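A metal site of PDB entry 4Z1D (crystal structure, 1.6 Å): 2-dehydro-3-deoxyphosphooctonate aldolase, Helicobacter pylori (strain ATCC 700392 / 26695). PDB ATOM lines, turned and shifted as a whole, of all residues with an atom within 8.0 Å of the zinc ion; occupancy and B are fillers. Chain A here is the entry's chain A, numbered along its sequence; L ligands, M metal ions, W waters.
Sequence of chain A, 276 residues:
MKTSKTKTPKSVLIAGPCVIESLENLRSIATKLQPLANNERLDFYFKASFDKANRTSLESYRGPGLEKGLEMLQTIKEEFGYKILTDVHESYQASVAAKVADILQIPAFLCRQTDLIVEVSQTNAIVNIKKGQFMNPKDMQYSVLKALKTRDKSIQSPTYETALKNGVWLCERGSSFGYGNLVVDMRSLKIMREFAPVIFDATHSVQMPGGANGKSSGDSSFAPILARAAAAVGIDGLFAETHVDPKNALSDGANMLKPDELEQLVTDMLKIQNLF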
ATOM      1  N   GLY A  16     -12.546   7.118  -2.595  1.00  0.00           N
ATOM      2  CA  GLY A  16     -12.900   8.283  -1.803  1.00  0.00           C
ATOM      3  C   GLY A  16     -13.137   9.473  -2.716  1.00  0.00           C
ATOM      4  O   GLY A  16     -13.085   9.323  -3.947  1.00  0.00           O
ATOM      5  N   PRO A  17     -13.401  10.643  -2.141  1.00  0.00           N
ATOM      6  CA  PRO A  17     -13.684  11.826  -2.933  1.00  0.00           C
ATOM      7  C   PRO A  17     -12.430  12.382  -3.587  1.00  0.00           C
ATOM      8  O   PRO A  17     -11.323  12.165  -3.093  1.00  0.00           O
ATOM      9  CB  PRO A  17     -14.236  12.805  -1.896  1.00  0.00           C
ATOM     10  CG  PRO A  17     -13.520  12.448  -0.637  1.00  0.00           C
ATOM     11  CD  PRO A  17     -13.311  10.955  -0.697  1.00  0.00           C
ATOM     12  N   CYS A  18     -12.604  13.085  -4.692  1.00  0.00           N
ATOM     13  CA  CYS A  18     -11.469  13.672  -5.404  1.00  0.00           C
ATOM     14  C   CYS A  18     -10.685  14.581  -4.488  1.00  0.00           C
ATOM     15  O   CYS A  18      -9.461  14.471  -4.383  1.00  0.00           O
ATOM     16  CB  CYS A  18     -11.960  14.442  -6.619  1.00  0.00           C
ATOM     17  SG  CYS A  18     -10.656  14.905  -7.766  1.00  0.00           S
ATOM     18  N   VAL A  19     -11.398  15.477  -3.812  1.00  0.00           N
ATOM     19  CA  VAL A  19     -10.791  16.452  -2.922  1.00  0.00           C
ATOM     20  C   VAL A  19     -11.435  16.390  -1.527  1.00  0.00           C
ATOM     21  O   VAL A  19     -12.584  15.969  -1.381  1.00  0.00           O
ATOM     22  CB  VAL A  19     -10.911  17.889  -3.497  1.00  0.00           C
ATOM     23  CG1 VAL A  19     -12.337  18.413  -3.399  1.00  0.00           C
ATOM     24  CG2 VAL A  19      -9.939  18.827  -2.798  1.00  0.00           C
ATOM     25  N   LYS A  47      -9.088   7.432  -0.167  1.00  0.00           N
ATOM     26  CA  LYS A  47      -8.387   8.474  -0.910  1.00  0.00           C
ATOM     27  C   LYS A  47      -9.076   9.826  -0.789  1.00  0.00           C
ATOM     28  O   LYS A  47     -10.288   9.917  -0.891  1.00  0.00           O
ATOM     29  CB  LYS A  47      -8.327   8.090  -2.407  1.00  0.00           C
ATOM     30  CG  LYS A  47      -7.492   9.000  -3.298  1.00  0.00           C
ATOM     31  CD  LYS A  47      -8.248  10.127  -4.006  1.00  0.00           C
ATOM     32  CE  LYS A  47      -7.279  11.030  -4.763  1.00  0.00           C
ATOM     33  NZ  LYS A  47      -7.918  12.074  -5.619  1.00  0.00           N
ATOM     34  N   SER A  49      -7.603  14.041  -1.927  1.00  0.00           N
ATOM     35  CA  SER A  49      -6.536  15.021  -2.150  1.00  0.00           C
ATOM     36  C   SER A  49      -6.693  16.198  -1.199  1.00  0.00           C
ATOM     37  O   SER A  49      -7.784  16.733  -1.038  1.00  0.00           O
ATOM     38  CB  SER A  49      -6.579  15.530  -3.581  1.00  0.00           C
ATOM     39  OG  SER A  49      -6.374  14.481  -4.508  1.00  0.00           O
ATOM     40  N   LYS A  52      -5.773  20.388  -4.950  1.00  0.00           N
ATOM     41  CA  LYS A  52      -5.930  20.253  -6.391  1.00  0.00           C
ATOM     42  C   LYS A  52      -5.103  21.376  -7.009  1.00  0.00           C
ATOM     43  O   LYS A  52      -5.483  22.538  -6.975  1.00  0.00           O
ATOM     44  CB  LYS A  52      -7.397  20.367  -6.803  1.00  0.00           C
ATOM     45  CG  LYS A  52      -8.346  19.452  -6.026  1.00  0.00           C
ATOM     46  CD  LYS A  52      -7.899  18.008  -5.955  1.00  0.00           C
ATOM     47  CE  LYS A  52      -7.886  17.324  -7.310  1.00  0.00           C
ATOM     48  NZ  LYS A  52      -7.481  15.896  -7.185  1.00  0.00           N
ATOM     49  N   LYS A 130       1.303   7.525 -10.835  1.00  0.00           N
ATOM     50  CA  LYS A 130       0.361   7.713 -11.957  1.00  0.00           C
ATOM     51  C   LYS A 130       1.139   7.835 -13.255  1.00  0.00           C
ATOM     52  O   LYS A 130       2.082   8.640 -13.344  1.00  0.00           O
ATOM     53  CB  LYS A 130      -0.498   8.961 -11.755  1.00  0.00           C
ATOM     54  CG  LYS A 130      -1.549   8.935 -10.629  1.00  0.00           C
ATOM     55  CD  LYS A 130      -2.697   7.989 -10.954  1.00  0.00           C
ATOM     56  CE  LYS A 130      -3.964   8.266 -10.166  1.00  0.00           C
ATOM     57  NZ  LYS A 130      -4.771   9.400 -10.688  1.00  0.00           N
ATOM     58  N   ARG A 173      -4.013   5.681 -16.057  1.00  0.00           N
ATOM     59  CA  ARG A 173      -5.091   6.673 -16.038  1.00  0.00           C
ATOM     60  C   ARG A 173      -5.395   7.269 -17.428  1.00  0.00           C
ATOM     61  O   ARG A 173      -5.987   8.350 -17.534  1.00  0.00           O
ATOM     62  CB  ARG A 173      -4.789   7.795 -15.023  1.00  0.00           C
ATOM     63  CG  ARG A 173      -3.578   8.680 -15.321  1.00  0.00           C
ATOM     64  CD  ARG A 173      -3.912  10.146 -15.114  1.00  0.00           C
ATOM     65  NE  ARG A 173      -4.837  10.645 -16.122  1.00  0.00           N
ATOM     66  CZ  ARG A 173      -5.656  11.679 -15.967  1.00  0.00           C
ATOM     67  NH1 ARG A 173      -6.436  11.989 -16.969  1.00  0.00           N
ATOM     68  NH2 ARG A 173      -5.714  12.383 -14.841  1.00  0.00           N
ATOM     69  N   ASP A 201      -6.992   3.416 -12.657  1.00  0.00           N
ATOM     70  CA  ASP A 201      -7.793   4.584 -12.276  1.00  0.00           C
ATOM     71  C   ASP A 201      -8.988   4.687 -13.227  1.00  0.00           C
ATOM     72  O   ASP A 201      -8.841   5.098 -14.387  1.00  0.00           O
ATOM     73  CB  ASP A 201      -6.914   5.849 -12.310  1.00  0.00           C
ATOM     74  CG  ASP A 201      -7.658   7.127 -12.015  1.00  0.00           C
ATOM     75  OD1 ASP A 201      -8.909   7.170 -12.017  1.00  0.00           O
ATOM     76  OD2 ASP A 201      -6.954   8.146 -11.801  1.00  0.00           O
ATOM     77  N   THR A 203     -11.667   6.571 -12.856  1.00  0.00           N
ATOM     78  CA  THR A 203     -12.306   7.876 -12.769  1.00  0.00           C
ATOM     79  C   THR A 203     -11.735   8.895 -13.739  1.00  0.00           C
ATOM     80  O   THR A 203     -12.487   9.548 -14.450  1.00  0.00           O
ATOM     81  CB  THR A 203     -12.134   8.484 -11.353  1.00  0.00           C
ATOM     82  OG1 THR A 203     -12.680   7.586 -10.393  1.00  0.00           O
ATOM     83  CG2 THR A 203     -12.831   9.841 -11.230  1.00  0.00           C
ATOM     84  N   HIS A 204     -10.421   9.049 -13.732  1.00  0.00           N
ATOM     85  CA  HIS A 204      -9.781  10.112 -14.495  1.00  0.00           C
ATOM     86  C   HIS A 204      -9.428   9.707 -15.912  1.00  0.00           C
ATOM     87  O   HIS A 204      -8.900  10.524 -16.653  1.00  0.00           O
ATOM     88  CB  HIS A 204      -8.520  10.600 -13.803  1.00  0.00           C
ATOM     89  CG  HIS A 204      -8.747  11.101 -12.412  1.00  0.00           C
ATOM     90  ND1 HIS A 204      -8.208  10.494 -11.310  1.00  0.00           N
ATOM     91  CD2 HIS A 204      -9.472  12.144 -11.957  1.00  0.00           C
ATOM     92  CE1 HIS A 204      -8.576  11.141 -10.217  1.00  0.00           C
ATOM     93  NE2 HIS A 204      -9.343  12.153 -10.583  1.00  0.00           N
ATOM     94  N   PHE A 239      -8.629   2.020  -8.647  1.00  0.00           N
ATOM     95  CA  PHE A 239      -8.741   3.364  -8.092  1.00  0.00           C
ATOM     96  C   PHE A 239     -10.023   3.971  -8.668  1.00  0.00           C
ATOM     97  O   PHE A 239     -10.191   4.035  -9.885  1.00  0.00           O
ATOM     98  CB  PHE A 239      -7.485   4.153  -8.495  1.00  0.00           C
ATOM     99  CG  PHE A 239      -7.484   5.610  -8.126  1.00  0.00           C
ATOM    100  CD1 PHE A 239      -8.362   6.514  -8.738  1.00  0.00           C
ATOM    101  CD2 PHE A 239      -6.542   6.107  -7.228  1.00  0.00           C
ATOM    102  CE1 PHE A 239      -8.316   7.864  -8.426  1.00  0.00           C
ATOM    103  CE2 PHE A 239      -6.494   7.461  -6.928  1.00  0.00           C
ATOM    104  CZ  PHE A 239      -7.390   8.334  -7.522  1.00  0.00           C
ATOM    105  N   ALA A 240     -10.955   4.369  -7.802  1.00  0.00           N
ATOM    106  CA  ALA A 240     -12.201   4.970  -8.265  1.00  0.00           C
ATOM    107  C   ALA A 240     -12.697   5.968  -7.255  1.00  0.00           C
ATOM    108  O   ALA A 240     -12.936   5.598  -6.087  1.00  0.00           O
ATOM    109  CB  ALA A 240     -13.245   3.903  -8.504  1.00  0.00           C
ATOM    110  N   GLU A 241     -12.905   7.208  -7.678  1.00  0.00           N
ATOM    111  CA  GLU A 241     -13.422   8.238  -6.786  1.00  0.00           C
ATOM    112  C   GLU A 241     -14.939   8.137  -6.623  1.00  0.00           C
ATOM    113  O   GLU A 241     -15.679   7.825  -7.565  1.00  0.00           O
ATOM    114  CB  GLU A 241     -12.989   9.626  -7.242  1.00  0.00           C
ATOM    115  CG  GLU A 241     -11.480   9.771  -7.159  1.00  0.00           C
ATOM    116  CD  GLU A 241     -10.956  11.065  -7.738  1.00  0.00           C
ATOM    117  OE1 GLU A 241     -11.659  11.723  -8.550  1.00  0.00           O
ATOM    118  OE2 GLU A 241      -9.802  11.421  -7.397  1.00  0.00           O
ATOM    119  N   THR A 242     -15.380   8.406  -5.394  1.00  0.00           N
ATOM    120  CA  THR A 242     -16.765   8.216  -4.998  1.00  0.00           C
ATOM    121  C   THR A 242     -17.174   9.332  -4.054  1.00  0.00           C
ATOM    122  O   THR A 242     -16.349   9.847  -3.299  1.00  0.00           O
ATOM    123  CB  THR A 242     -16.972   6.828  -4.354  1.00  0.00           C
ATOM    124  OG1 THR A 242     -18.361   6.645  -4.016  1.00  0.00           O
ATOM    125  CG2 THR A 242     -16.114   6.662  -3.095  1.00  0.00           C
ATOM    126  N   SER A 251     -15.029  18.922  -6.581  1.00  0.00           N
ATOM    127  CA  SER A 251     -14.095  18.532  -7.631  1.00  0.00           C
ATOM    128  C   SER A 251     -14.518  17.190  -8.214  1.00  0.00           C
ATOM    129  O   SER A 251     -14.838  16.261  -7.451  1.00  0.00           O
ATOM    130  CB  SER A 251     -12.663  18.426  -7.085  1.00  0.00           C
ATOM    131  OG  SER A 251     -11.731  18.084  -8.119  1.00  0.00           O
ATOM    132  N   ASP A 252     -14.542  17.090  -9.537  1.00  0.00           N
ATOM    133  CA  ASP A 252     -14.819  15.841 -10.242  1.00  0.00           C
ATOM    134  C   ASP A 252     -16.214  15.251 -10.021  1.00  0.00           C
ATOM    135  O   ASP A 252     -16.417  14.057 -10.186  1.00  0.00           O
ATOM    136  CB  ASP A 252     -13.726  14.791  -9.905  1.00  0.00           C
ATOM    137  CG  ASP A 252     -12.848  14.455 -11.091  1.00  0.00           C
ATOM    138  OD1 ASP A 252     -13.113  14.951 -12.197  1.00  0.00           O
ATOM    139  OD2 ASP A 252     -11.882  13.675 -10.909  1.00  0.00           O
ATOM    140  N   GLY A 253     -17.182  16.100  -9.685  1.00  0.00           N
ATOM    141  CA  GLY A 253     -18.557  15.661  -9.470  1.00  0.00           C
ATOM    142  C   GLY A 253     -19.108  14.858 -10.626  1.00  0.00           C
ATOM    143  O   GLY A 253     -19.755  13.835 -10.419  1.00  0.00           O
ATOM    144  N   ASN A 255     -17.683  12.901 -12.686  1.00  0.00           N
ATOM    145  CA  ASN A 255     -17.025  11.624 -12.926  1.00  0.00           C
ATOM    146  C   ASN A 255     -16.964  10.660 -11.738  1.00  0.00           C
ATOM    147  O   ASN A 255     -16.494   9.536 -11.887  1.00  0.00           O
ATOM    148  CB  ASN A 255     -15.617  11.898 -13.442  1.00  0.00           C
ATOM    149  CG  ASN A 255     -15.641  12.538 -14.805  1.00  0.00           C
ATOM    150  OD1 ASN A 255     -16.024  11.912 -15.785  1.00  0.00           O
ATOM    151  ND2 ASN A 255     -15.256  13.812 -14.862  1.00  0.00           N
ATOM    152  N   MET A 256     -17.434  11.088 -10.569  1.00  0.00           N
ATOM    153  CA  MET A 256     -17.424  10.218  -9.398  1.00  0.00           C
ATOM    154  C   MET A 256     -18.646   9.300  -9.366  1.00  0.00           C
ATOM    155  O   MET A 256     -19.718   9.637  -9.884  1.00  0.00           O
ATOM    156  CB  MET A 256     -17.317  11.038  -8.116  1.00  0.00           C
ATOM    157  CG  MET A 256     -15.947  11.684  -7.931  1.00  0.00           C
ATOM    158  SD  MET A 256     -15.701  12.464  -6.324  1.00  0.00           S
ATOM    159  CE  MET A 256     -16.752  13.905  -6.474  1.00  0.00           C
HETATM  160  C1  LIG L   1      -5.728  12.421  -8.354  1.00  0.00           C
HETATM  161  O1  LIG L   1      -6.260  13.093  -7.435  1.00  0.00           O
HETATM  162  O2  LIG L   1      -5.762  11.162  -8.389  1.00  0.00           O
HETATM  163  C2  LIG L   1      -5.045  13.092  -9.450  1.00  0.00           C
HETATM  164  C3  LIG L   1      -4.822  14.393  -9.434  1.00  0.00           C
HETATM  165  O3  LIG L   1      -4.609  12.225 -10.531  1.00  0.00           O
HETATM  166  P1  LIG L   1      -3.630  12.582 -11.766  1.00  0.00           P
HETATM  167  O4  LIG L   1      -2.334  13.110 -11.170  1.00  0.00           O
HETATM  168  O5  LIG L   1      -3.538  11.217 -12.374  1.00  0.00           O
HETATM  169  O6  LIG L   1      -4.422  13.609 -12.547  1.00  0.00           O
HETATM  170 ZN    ZN M   1     -10.705  13.181  -9.307  1.00  0.00          ZN
HETATM  171  O   HOH W   1      -8.067  15.160  -9.960  1.00  0.00           O
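NZ of Lys 52 lies within salt-bridge range of O1 of the ligand (3.1 Å).
The side-chain amino group of Lys 47 lies within salt-bridge range of an oxygen (O1) of the ligand, 2.7 Å away.
The side-chain hydroxyl (OG) of Ser 49 lies within hydrogen-bond range of an oxygen (O1) of the ligand, at 3.2 Å.
The side-chain amino group of Lys 130 is in salt-bridge range of an oxygen (O5) of the ligand.
An oxygen (O6) of the ligand is in salt-bridge range of the guanidinium group of Arg 173 (2.9 Å).
N of Glu 241 lies within hydrogen-bond range of OG1 of Thr 203, at 2.8 Å.
The side-chain carboxylate (OE2) of Glu 241 is in salt-bridge range of the side-chain amino group (NZ) of Lys 47 (2.7 Å).
A ring nitrogen (ND1) of His 204 sits at hydrogen-bond distance from the side-chain carboxylate of Asp 201 (2.7 Å).
O of His 204 lies within hydrogen-bond range of NH1 of Arg 173 (2.9 Å).
The backbone carbonyl oxygen (O) of Cys 18 lies within hydrogen-bond range of the side-chain amino group (NZ) of Lys 47.
The side-chain hydroxyl of Ser 251 lies close to the side-chain sulfur of Cys 18 (3.4 Å).
The side-chain sulfur (SD) of Met 256 is in hydrogen-bond range of the backbone NH (N) of Cys 18, 3.6 Å away.
The backbone carbonyl oxygen of Cys 18 sits at hydrogen-bond distance from the side-chain hydroxyl of Ser 49 (3.1 Å).
Four residues have an atom within 4 Å of the zinc ion: Cys 18, His 204, Glu 241 and Asp 252.
Along chain A the residues within 4 Å of the zinc ion span positions 18 to 252.
The nearest printed residue that does not touch the zinc ion is Thr 203 (4.4 Å).
OE1 of Glu 241 binds the zinc ion (1.9 Å).
The side-chain carboxylate (OD2) of Asp 252 is bound to the zinc ion (2.0 Å).
NE2 of His 204 is bound to the zinc ion, 2.1 Å away.
The zinc ion is bound by SG of Cys 18 (2.3 Å).
Slightly farther from the zinc ion lies OE2 of Glu 241 (2.7 Å).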
